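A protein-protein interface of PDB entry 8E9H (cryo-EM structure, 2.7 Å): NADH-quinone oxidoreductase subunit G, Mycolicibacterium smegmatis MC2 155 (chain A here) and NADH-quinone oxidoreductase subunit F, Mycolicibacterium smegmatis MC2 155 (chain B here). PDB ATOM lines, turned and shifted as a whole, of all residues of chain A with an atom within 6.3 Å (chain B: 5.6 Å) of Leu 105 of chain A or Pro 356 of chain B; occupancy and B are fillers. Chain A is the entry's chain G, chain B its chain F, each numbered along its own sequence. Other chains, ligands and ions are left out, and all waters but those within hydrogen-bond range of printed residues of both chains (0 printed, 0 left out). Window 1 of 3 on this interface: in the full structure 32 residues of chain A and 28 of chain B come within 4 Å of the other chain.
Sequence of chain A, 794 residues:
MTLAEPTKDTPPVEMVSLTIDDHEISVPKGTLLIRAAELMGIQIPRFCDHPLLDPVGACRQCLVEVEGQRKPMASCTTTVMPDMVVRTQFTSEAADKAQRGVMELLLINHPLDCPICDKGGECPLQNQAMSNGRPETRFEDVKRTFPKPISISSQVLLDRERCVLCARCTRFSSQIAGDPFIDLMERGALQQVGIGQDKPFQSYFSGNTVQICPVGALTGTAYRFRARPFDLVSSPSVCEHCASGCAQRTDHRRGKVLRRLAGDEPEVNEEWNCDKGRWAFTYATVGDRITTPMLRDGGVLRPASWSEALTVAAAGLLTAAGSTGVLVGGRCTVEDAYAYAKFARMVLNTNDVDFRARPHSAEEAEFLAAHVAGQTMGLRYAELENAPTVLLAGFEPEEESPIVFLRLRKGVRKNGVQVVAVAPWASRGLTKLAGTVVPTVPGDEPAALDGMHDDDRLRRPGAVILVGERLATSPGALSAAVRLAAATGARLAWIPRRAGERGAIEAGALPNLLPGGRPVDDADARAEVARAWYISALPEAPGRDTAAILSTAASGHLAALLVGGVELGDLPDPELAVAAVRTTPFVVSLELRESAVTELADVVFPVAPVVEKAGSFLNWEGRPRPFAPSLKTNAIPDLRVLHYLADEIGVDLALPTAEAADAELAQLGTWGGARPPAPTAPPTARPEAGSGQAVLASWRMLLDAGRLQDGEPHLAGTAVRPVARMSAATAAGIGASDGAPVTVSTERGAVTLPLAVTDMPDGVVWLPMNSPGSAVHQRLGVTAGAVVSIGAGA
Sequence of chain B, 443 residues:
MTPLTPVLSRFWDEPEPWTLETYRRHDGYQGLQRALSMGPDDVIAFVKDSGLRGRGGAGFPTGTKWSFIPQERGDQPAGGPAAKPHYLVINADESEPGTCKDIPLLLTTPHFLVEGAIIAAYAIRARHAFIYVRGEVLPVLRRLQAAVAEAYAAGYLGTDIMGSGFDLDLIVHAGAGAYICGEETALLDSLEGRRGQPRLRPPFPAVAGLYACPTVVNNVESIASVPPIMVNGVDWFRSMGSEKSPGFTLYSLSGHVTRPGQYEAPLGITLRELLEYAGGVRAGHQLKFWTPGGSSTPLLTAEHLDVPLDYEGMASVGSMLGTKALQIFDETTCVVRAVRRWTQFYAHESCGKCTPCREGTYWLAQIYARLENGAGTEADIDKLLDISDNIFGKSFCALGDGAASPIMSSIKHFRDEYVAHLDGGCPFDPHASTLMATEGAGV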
ATOM      1  N   ALA A  58     -29.463   5.633 -15.446  1.00  0.00           N
ATOM      2  CA  ALA A  58     -29.717   6.372 -14.215  1.00  0.00           C
ATOM      3  C   ALA A  58     -29.708   5.452 -13.005  1.00  0.00           C
ATOM      4  O   ALA A  58     -28.927   5.647 -12.069  1.00  0.00           O
ATOM      5  CB  ALA A  58     -31.052   7.105 -14.318  1.00  0.00           C
ATOM      6  N   CYS A  59     -30.573   4.442 -13.001  1.00  0.00           N
ATOM      7  CA  CYS A  59     -30.764   3.640 -11.801  1.00  0.00           C
ATOM      8  C   CYS A  59     -29.516   2.872 -11.396  1.00  0.00           C
ATOM      9  O   CYS A  59     -29.392   2.513 -10.222  1.00  0.00           O
ATOM     10  CB  CYS A  59     -31.921   2.665 -12.004  1.00  0.00           C
ATOM     11  SG  CYS A  59     -31.528   1.251 -13.033  1.00  0.00           S
ATOM     12  N   ARG A  60     -28.596   2.615 -12.319  1.00  0.00           N
ATOM     13  CA  ARG A  60     -27.384   1.853 -12.039  1.00  0.00           C
ATOM     14  C   ARG A  60     -27.683   0.418 -11.635  1.00  0.00           C
ATOM     15  O   ARG A  60     -26.835  -0.248 -11.041  1.00  0.00           O
ATOM     16  CB  ARG A  60     -26.544   2.522 -10.948  1.00  0.00           C
ATOM     17  CG  ARG A  60     -26.331   4.005 -11.131  1.00  0.00           C
ATOM     18  CD  ARG A  60     -25.781   4.323 -12.500  1.00  0.00           C
ATOM     19  NE  ARG A  60     -24.485   3.697 -12.715  1.00  0.00           N
ATOM     20  CZ  ARG A  60     -23.883   3.614 -13.892  1.00  0.00           C
ATOM     21  NH1 ARG A  60     -24.434   4.110 -14.986  1.00  0.00           N
ATOM     22  NH2 ARG A  60     -22.698   3.018 -13.973  1.00  0.00           N
ATOM     23  N   LEU A  63     -25.679  -3.003 -13.641  1.00  0.00           N
ATOM     24  CA  LEU A  63     -24.225  -3.045 -13.660  1.00  0.00           C
ATOM     25  C   LEU A  63     -23.733  -4.462 -13.906  1.00  0.00           C
ATOM     26  O   LEU A  63     -24.275  -5.426 -13.360  1.00  0.00           O
ATOM     27  CB  LEU A  63     -23.669  -2.521 -12.342  1.00  0.00           C
ATOM     28  CG  LEU A  63     -23.957  -1.049 -12.075  1.00  0.00           C
ATOM     29  CD1 LEU A  63     -23.661  -0.706 -10.633  1.00  0.00           C
ATOM     30  CD2 LEU A  63     -23.147  -0.178 -13.007  1.00  0.00           C
ATOM     31  N   ARG A 100     -26.857  -5.968  -6.008  1.00  0.00           N
ATOM     32  CA  ARG A 100     -27.611  -6.107  -4.770  1.00  0.00           C
ATOM     33  C   ARG A 100     -27.511  -4.853  -3.917  1.00  0.00           C
ATOM     34  O   ARG A 100     -28.486  -4.461  -3.270  1.00  0.00           O
ATOM     35  CB  ARG A 100     -27.128  -7.328  -4.000  1.00  0.00           C
ATOM     36  CG  ARG A 100     -27.645  -8.615  -4.584  1.00  0.00           C
ATOM     37  CD  ARG A 100     -27.051  -9.825  -3.915  1.00  0.00           C
ATOM     38  NE  ARG A 100     -27.416 -11.035  -4.637  1.00  0.00           N
ATOM     39  CZ  ARG A 100     -28.598 -11.626  -4.545  1.00  0.00           C
ATOM     40  NH1 ARG A 100     -29.546 -11.157  -3.752  1.00  0.00           N
ATOM     41  NH2 ARG A 100     -28.836 -12.715  -5.271  1.00  0.00           N
ATOM     42  N   GLY A 101     -26.348  -4.207  -3.900  1.00  0.00           N
ATOM     43  CA  GLY A 101     -26.241  -2.941  -3.204  1.00  0.00           C
ATOM     44  C   GLY A 101     -27.138  -1.885  -3.814  1.00  0.00           C
ATOM     45  O   GLY A 101     -27.772  -1.102  -3.100  1.00  0.00           O
ATOM     46  N   VAL A 102     -27.209  -1.848  -5.144  1.00  0.00           N
ATOM     47  CA  VAL A 102     -28.098  -0.900  -5.801  1.00  0.00           C
ATOM     48  C   VAL A 102     -29.545  -1.201  -5.447  1.00  0.00           C
ATOM     49  O   VAL A 102     -30.332  -0.289  -5.185  1.00  0.00           O
ATOM     50  CB  VAL A 102     -27.874  -0.916  -7.320  1.00  0.00           C
ATOM     51  CG1 VAL A 102     -28.936  -0.089  -8.009  1.00  0.00           C
ATOM     52  CG2 VAL A 102     -26.501  -0.383  -7.650  1.00  0.00           C
ATOM     53  N   MET A 103     -29.926  -2.477  -5.439  1.00  0.00           N
ATOM     54  CA  MET A 103     -31.293  -2.824  -5.063  1.00  0.00           C
ATOM     55  C   MET A 103     -31.591  -2.397  -3.633  1.00  0.00           C
ATOM     56  O   MET A 103     -32.661  -1.842  -3.351  1.00  0.00           O
ATOM     57  CB  MET A 103     -31.513  -4.325  -5.229  1.00  0.00           C
ATOM     58  CG  MET A 103     -32.900  -4.798  -4.838  1.00  0.00           C
ATOM     59  SD  MET A 103     -34.202  -4.031  -5.809  1.00  0.00           S
ATOM     60  CE  MET A 103     -33.830  -4.685  -7.428  1.00  0.00           C
ATOM     61  N   GLU A 104     -30.659  -2.648  -2.716  1.00  0.00           N
ATOM     62  CA  GLU A 104     -30.844  -2.215  -1.337  1.00  0.00           C
ATOM     63  C   GLU A 104     -31.061  -0.713  -1.269  1.00  0.00           C
ATOM     64  O   GLU A 104     -32.034  -0.241  -0.674  1.00  0.00           O
ATOM     65  CB  GLU A 104     -29.635  -2.625  -0.500  1.00  0.00           C
ATOM     66  CG  GLU A 104     -29.628  -2.061   0.908  1.00  0.00           C
ATOM     67  CD  GLU A 104     -28.395  -2.463   1.684  1.00  0.00           C
ATOM     68  OE1 GLU A 104     -27.309  -2.536   1.075  1.00  0.00           O
ATOM     69  OE2 GLU A 104     -28.508  -2.698   2.905  1.00  0.00           O
ATOM     70  N   LEU A 105     -30.167   0.058  -1.890  1.00  0.00           N
ATOM     71  CA  LEU A 105     -30.322   1.507  -1.883  1.00  0.00           C
ATOM     72  C   LEU A 105     -31.624   1.925  -2.544  1.00  0.00           C
ATOM     73  O   LEU A 105     -32.175   2.982  -2.227  1.00  0.00           O
ATOM     74  CB  LEU A 105     -29.139   2.162  -2.588  1.00  0.00           C
ATOM     75  CG  LEU A 105     -27.792   1.982  -1.896  1.00  0.00           C
ATOM     76  CD1 LEU A 105     -26.690   2.566  -2.744  1.00  0.00           C
ATOM     77  CD2 LEU A 105     -27.802   2.623  -0.526  1.00  0.00           C
ATOM     78  N   LEU A 106     -32.125   1.111  -3.467  1.00  0.00           N
ATOM     79  CA  LEU A 106     -33.390   1.409  -4.116  1.00  0.00           C
ATOM     80  C   LEU A 106     -34.564   1.175  -3.181  1.00  0.00           C
ATOM     81  O   LEU A 106     -35.589   1.852  -3.295  1.00  0.00           O
ATOM     82  CB  LEU A 106     -33.526   0.549  -5.369  1.00  0.00           C
ATOM     83  CG  LEU A 106     -34.377   1.070  -6.519  1.00  0.00           C
ATOM     84  CD1 LEU A 106     -33.768   2.297  -7.144  1.00  0.00           C
ATOM     85  CD2 LEU A 106     -34.527  -0.018  -7.557  1.00  0.00           C
ATOM     86  N   LEU A 107     -34.436   0.229  -2.254  1.00  0.00           N
ATOM     87  CA  LEU A 107     -35.554  -0.144  -1.401  1.00  0.00           C
ATOM     88  C   LEU A 107     -35.597   0.598  -0.075  1.00  0.00           C
ATOM     89  O   LEU A 107     -36.623   0.538   0.610  1.00  0.00           O
ATOM     90  CB  LEU A 107     -35.519  -1.645  -1.108  1.00  0.00           C
ATOM     91  CG  LEU A 107     -35.945  -2.562  -2.249  1.00  0.00           C
ATOM     92  CD1 LEU A 107     -35.725  -4.007  -1.863  1.00  0.00           C
ATOM     93  CD2 LEU A 107     -37.391  -2.329  -2.612  1.00  0.00           C
ATOM     94  N   ILE A 108     -34.527   1.286   0.320  1.00  0.00           N
ATOM     95  CA  ILE A 108     -34.508   1.875   1.656  1.00  0.00           C
ATOM     96  C   ILE A 108     -35.620   2.903   1.802  1.00  0.00           C
ATOM     97  O   ILE A 108     -36.341   2.919   2.807  1.00  0.00           O
ATOM     98  CB  ILE A 108     -33.130   2.483   1.969  1.00  0.00           C
ATOM     99  CG1 ILE A 108     -32.754   3.553   0.950  1.00  0.00           C
ATOM    100  CG2 ILE A 108     -32.076   1.402   2.005  1.00  0.00           C
ATOM    101  CD1 ILE A 108     -31.410   4.169   1.206  1.00  0.00           C
ATOM    102  N   ASN A 109     -35.787   3.767   0.809  1.00  0.00           N
ATOM    103  CA  ASN A 109     -36.789   4.819   0.867  1.00  0.00           C
ATOM    104  C   ASN A 109     -38.149   4.371   0.358  1.00  0.00           C
ATOM    105  O   ASN A 109     -39.112   5.136   0.456  1.00  0.00           O
ATOM    106  CB  ASN A 109     -36.320   6.026   0.056  1.00  0.00           C
ATOM    107  CG  ASN A 109     -35.547   7.018   0.888  1.00  0.00           C
ATOM    108  OD1 ASN A 109     -35.812   7.192   2.074  1.00  0.00           O
ATOM    109  ND2 ASN A 109     -34.580   7.678   0.268  1.00  0.00           N
ATOM    110  N   CYS B 354     -28.669   9.363 -10.044  1.00  0.00           N
ATOM    111  CA  CYS B 354     -28.267   8.029  -9.638  1.00  0.00           C
ATOM    112  C   CYS B 354     -29.205   7.470  -8.582  1.00  0.00           C
ATOM    113  O   CYS B 354     -29.845   8.202  -7.825  1.00  0.00           O
ATOM    114  CB  CYS B 354     -26.864   8.037  -9.051  1.00  0.00           C
ATOM    115  SG  CYS B 354     -25.568   8.109 -10.236  1.00  0.00           S
ATOM    116  N   THR B 355     -29.274   6.143  -8.533  1.00  0.00           N
ATOM    117  CA  THR B 355     -29.717   5.502  -7.298  1.00  0.00           C
ATOM    118  C   THR B 355     -28.584   5.457  -6.290  1.00  0.00           C
ATOM    119  O   THR B 355     -28.797   5.861  -5.132  1.00  0.00           O
ATOM    120  CB  THR B 355     -30.264   4.107  -7.591  1.00  0.00           C
ATOM    121  OG1 THR B 355     -31.241   4.185  -8.633  1.00  0.00           O
ATOM    122  CG2 THR B 355     -30.892   3.524  -6.346  1.00  0.00           C
ATOM    123  N   PRO B 356     -27.372   5.018  -6.642  1.00  0.00           N
ATOM    124  CA  PRO B 356     -26.306   4.997  -5.633  1.00  0.00           C
ATOM    125  C   PRO B 356     -26.105   6.336  -4.958  1.00  0.00           C
ATOM    126  O   PRO B 356     -26.318   6.443  -3.752  1.00  0.00           O
ATOM    127  CB  PRO B 356     -25.080   4.566  -6.444  1.00  0.00           C
ATOM    128  CG  PRO B 356     -25.631   3.778  -7.541  1.00  0.00           C
ATOM    129  CD  PRO B 356     -26.908   4.451  -7.918  1.00  0.00           C
ATOM    130  N   CYS B 357     -25.748   7.379  -5.699  1.00  0.00           N
ATOM    131  CA  CYS B 357     -25.443   8.641  -5.038  1.00  0.00           C
ATOM    132  C   CYS B 357     -26.638   9.141  -4.241  1.00  0.00           C
ATOM    133  O   CYS B 357     -26.532   9.365  -3.033  1.00  0.00           O
ATOM    134  CB  CYS B 357     -24.997   9.676  -6.063  1.00  0.00           C
ATOM    135  SG  CYS B 357     -24.904  11.363  -5.440  1.00  0.00           S
ATOM    136  N   ARG B 358     -27.802   9.255  -4.877  1.00  0.00           N
ATOM    137  CA  ARG B 358     -28.964   9.804  -4.188  1.00  0.00           C
ATOM    138  C   ARG B 358     -29.267   9.028  -2.911  1.00  0.00           C
ATOM    139  O   ARG B 358     -29.139   9.549  -1.793  1.00  0.00           O
ATOM    140  CB  ARG B 358     -30.171   9.784  -5.125  1.00  0.00           C
ATOM    141  CG  ARG B 358     -31.478  10.150  -4.451  1.00  0.00           C
ATOM    142  CD  ARG B 358     -32.641  10.206  -5.425  1.00  0.00           C
ATOM    143  NE  ARG B 358     -32.408   9.425  -6.634  1.00  0.00           N
ATOM    144  CZ  ARG B 358     -32.887   8.209  -6.854  1.00  0.00           C
ATOM    145  NH1 ARG B 358     -33.589   7.564  -5.939  1.00  0.00           N
ATOM    146  NH2 ARG B 358     -32.653   7.623  -8.023  1.00  0.00           N
ATOM    147  N   GLU B 359     -29.661   7.765  -3.063  1.00  0.00           N
ATOM    148  CA  GLU B 359     -30.115   6.980  -1.928  1.00  0.00           C
ATOM    149  C   GLU B 359     -29.011   6.746  -0.907  1.00  0.00           C
ATOM    150  O   GLU B 359     -29.253   6.858   0.300  1.00  0.00           O
ATOM    151  CB  GLU B 359     -30.671   5.640  -2.412  1.00  0.00           C
ATOM    152  N   GLY B 360     -27.800   6.418  -1.355  1.00  0.00           N
ATOM    153  CA  GLY B 360     -26.725   6.152  -0.423  1.00  0.00           C
ATOM    154  C   GLY B 360     -26.294   7.375   0.356  1.00  0.00           C
ATOM    155  O   GLY B 360     -25.982   7.274   1.539  1.00  0.00           O
ATOM    156  N   THR B 361     -26.241   8.542  -0.287  1.00  0.00           N
ATOM    157  CA  THR B 361     -25.923   9.750   0.461  1.00  0.00           C
ATOM    158  C   THR B 361     -27.011  10.060   1.472  1.00  0.00           C
ATOM    159  O   THR B 361     -26.717  10.456   2.603  1.00  0.00           O
ATOM    160  CB  THR B 361     -25.721  10.926  -0.486  1.00  0.00           C
ATOM    161  OG1 THR B 361     -26.874  11.070  -1.323  1.00  0.00           O
ATOM    162  CG2 THR B 361     -24.485  10.719  -1.337  1.00  0.00           C
ATOM    163  N   TRP B 363     -28.868   7.862   3.012  1.00  0.00           N
ATOM    164  CA  TRP B 363     -28.690   6.895   4.087  1.00  0.00           C
ATOM    165  C   TRP B 363     -27.476   7.229   4.942  1.00  0.00           C
ATOM    166  O   TRP B 363     -27.525   7.136   6.172  1.00  0.00           O
ATOM    167  CB  TRP B 363     -28.555   5.498   3.487  1.00  0.00           C
ATOM    168  CG  TRP B 363     -28.753   4.391   4.450  1.00  0.00           C
ATOM    169  CD1 TRP B 363     -29.129   4.490   5.752  1.00  0.00           C
ATOM    170  CD2 TRP B 363     -28.589   2.999   4.184  1.00  0.00           C
ATOM    171  NE1 TRP B 363     -29.207   3.245   6.317  1.00  0.00           N
ATOM    172  CE2 TRP B 363     -28.879   2.310   5.371  1.00  0.00           C
ATOM    173  CE3 TRP B 363     -28.224   2.267   3.054  1.00  0.00           C
ATOM    174  CZ2 TRP B 363     -28.817   0.928   5.463  1.00  0.00           C
ATOM    175  CZ3 TRP B 363     -28.162   0.898   3.145  1.00  0.00           C
ATOM    176  CH2 TRP B 363     -28.456   0.241   4.341  1.00  0.00           C
ATOM    177  N   ILE B 387     -22.053   0.610   2.526  1.00  0.00           N
ATOM    178  CA  ILE B 387     -22.796   1.579   1.731  1.00  0.00           C
ATOM    179  C   ILE B 387     -21.847   2.389   0.865  1.00  0.00           C
ATOM    180  O   ILE B 387     -22.106   2.612  -0.322  1.00  0.00           O
ATOM    181  CB  ILE B 387     -23.635   2.489   2.643  1.00  0.00           C
ATOM    182  CG1 ILE B 387     -24.725   1.681   3.341  1.00  0.00           C
ATOM    183  CG2 ILE B 387     -24.248   3.614   1.840  1.00  0.00           C
ATOM    184  CD1 ILE B 387     -25.239   2.330   4.593  1.00  0.00           C
ATOM    185  N   ASN B 390     -20.830   0.371  -1.972  1.00  0.00           N
ATOM    186  CA  ASN B 390     -21.919   0.296  -2.937  1.00  0.00           C
ATOM    187  C   ASN B 390     -22.127   1.601  -3.689  1.00  0.00           C
ATOM    188  O   ASN B 390     -22.777   1.590  -4.738  1.00  0.00           O
ATOM    189  CB  ASN B 390     -23.216  -0.093  -2.235  1.00  0.00           C
ATOM    190  CG  ASN B 390     -23.193  -1.511  -1.717  1.00  0.00           C
ATOM    191  OD1 ASN B 390     -22.393  -2.332  -2.160  1.00  0.00           O
ATOM    192  ND2 ASN B 390     -24.075  -1.810  -0.773  1.00  0.00           N
ATOM    193  N   ILE B 391     -21.618   2.717  -3.177  1.00  0.00           N
ATOM    194  CA  ILE B 391     -21.724   3.992  -3.875  1.00  0.00           C
ATOM    195  C   ILE B 391     -20.505   4.165  -4.764  1.00  0.00           C
ATOM    196  O   ILE B 391     -20.627   4.467  -5.955  1.00  0.00           O
ATOM    197  CB  ILE B 391     -21.846   5.168  -2.891  1.00  0.00           C
ATOM    198  CG1 ILE B 391     -23.167   5.095  -2.133  1.00  0.00           C
ATOM    199  CG2 ILE B 391     -21.731   6.485  -3.634  1.00  0.00           C
ATOM    200  CD1 ILE B 391     -23.268   6.099  -1.019  1.00  0.00           C
ATOM    201  N   LYS B 394     -20.055   2.751  -8.470  1.00  0.00           N
ATOM    202  CA  LYS B 394     -21.339   2.381  -9.049  1.00  0.00           C
ATOM    203  C   LYS B 394     -22.140   3.578  -9.530  1.00  0.00           C
ATOM    204  O   LYS B 394     -23.025   3.421 -10.376  1.00  0.00           O
ATOM    205  CB  LYS B 394     -22.178   1.603  -8.032  1.00  0.00           C
ATOM    206  CG  LYS B 394     -21.388   0.689  -7.117  1.00  0.00           C
ATOM    207  CD  LYS B 394     -20.522  -0.279  -7.891  1.00  0.00           C
ATOM    208  CE  LYS B 394     -19.892  -1.301  -6.967  1.00  0.00           C
ATOM    209  NZ  LYS B 394     -18.853  -0.693  -6.098  1.00  0.00           N
ATOM    210  N   SER B 395     -21.857   4.769  -9.018  1.00  0.00           N
ATOM    211  CA  SER B 395     -22.659   5.929  -9.363  1.00  0.00           C
ATOM    212  C   SER B 395     -22.368   6.385 -10.789  1.00  0.00           C
ATOM    213  O   SER B 395     -21.376   5.998 -11.409  1.00  0.00           O
ATOM    214  CB  SER B 395     -22.398   7.063  -8.381  1.00  0.00           C
ATOM    215  OG  SER B 395     -21.121   7.630  -8.592  1.00  0.00           O
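The backbone carbonyl oxygen (O) of Cys 59 of chain A lies within hydrogen-bond range of the side-chain hydroxyl (OG1) of Thr 355 of chain B (3.0 Å).
The backbone carbonyl oxygen (O) of Lys 394 of chain B lies within hydrogen-bond range of the guanidinium group (NE) of Arg 60 of chain A, at 2.8 Å.
O of Cys 354 of chain B is in hydrogen-bond range of NH2 of Arg 358 of chain B (2.9 Å).
N of Thr 355 of chain B touches O of Ala 58 of chain A, 3.6 Å away.
Cys 59 of chain A touches Pro 356 of chain B (O to CD, 3.9 Å).
CD1 of Leu 63 of chain A touches CB of Lys 394 of chain B, 3.8 Å away.
Glu 104 of chain A touches Trp 363 of chain B (OE2 to CH2, 3.3 Å).
OE1 of Glu 104 of chain A touches ND2 of Asn 390 of chain B, at 3.8 Å.
Pro 356 of chain B touches Leu 105 of chain A.
Leu 105 of chain A touches Glu 359 of chain B.
CD2 of Leu 105 of chain A touches CA of Gly 360 of chain B, at 3.7 Å.
Trp 363 of chain B touches Leu 105 of chain A (CE3 to CD2, 3.6 Å).
CD1 of Leu 106 of chain A touches CG2 of Thr 355 of chain B (3.2 Å).
Of the printed residues of chain B, Cys 59 of chain A touches Thr 355 (3.0 Å) and Pro 356 (3.9 Å).
Printed residues of chain B within 4 Å of Gly 101 of chain A: Asn 390 (3.4 Å).
Of chain B, only Pro 356 (3.8 Å), Glu 359 (3.1 Å), Gly 360 (3.7 Å) and Trp 363 (3.6 Å) come within 4 Å of Leu 105 of chain A.
Printed residues of chain B within 4 Å of Leu 106 of chain A: Thr 355 (3.2 Å).
Of chain A, only Cys 59 (3.9 Å), Arg 60 (3.3 Å) and Leu 105 (3.8 Å) come within 4 Å of Pro 356 of chain B.
Of the printed residues of chain A, Gly 360 of chain B touches Leu 105.
The nearest residue of chain A that does not touch Pro 356 of chain B is Val 102 of chain A (4.3 Å).
The nearest printed residue of chain B that does not touch Gly 101 of chain A is Thr 355 of chain B (6.5 Å).
Of the 14 printed residues of chain A, 9 touch a printed residue of chain B.
Printed residues of chain A that touch a printed residue of chain B: Ala 58, Cys 59, Arg 60, Leu 63, Gly 101, Glu 104, Leu 105, Leu 106 and Ile 108.
Hydrophobic or aromatic side chains of chain A that line the printed part of chain B: Leu 63, Leu 105, Leu 106 and Ile 108.
Among the printed residues, 18 pairs touch across the chains.
Among the printed residues, no Asp or Glu carboxylate lies within 4 Å of a Lys or Arg side-chain nitrogen of the other chain.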
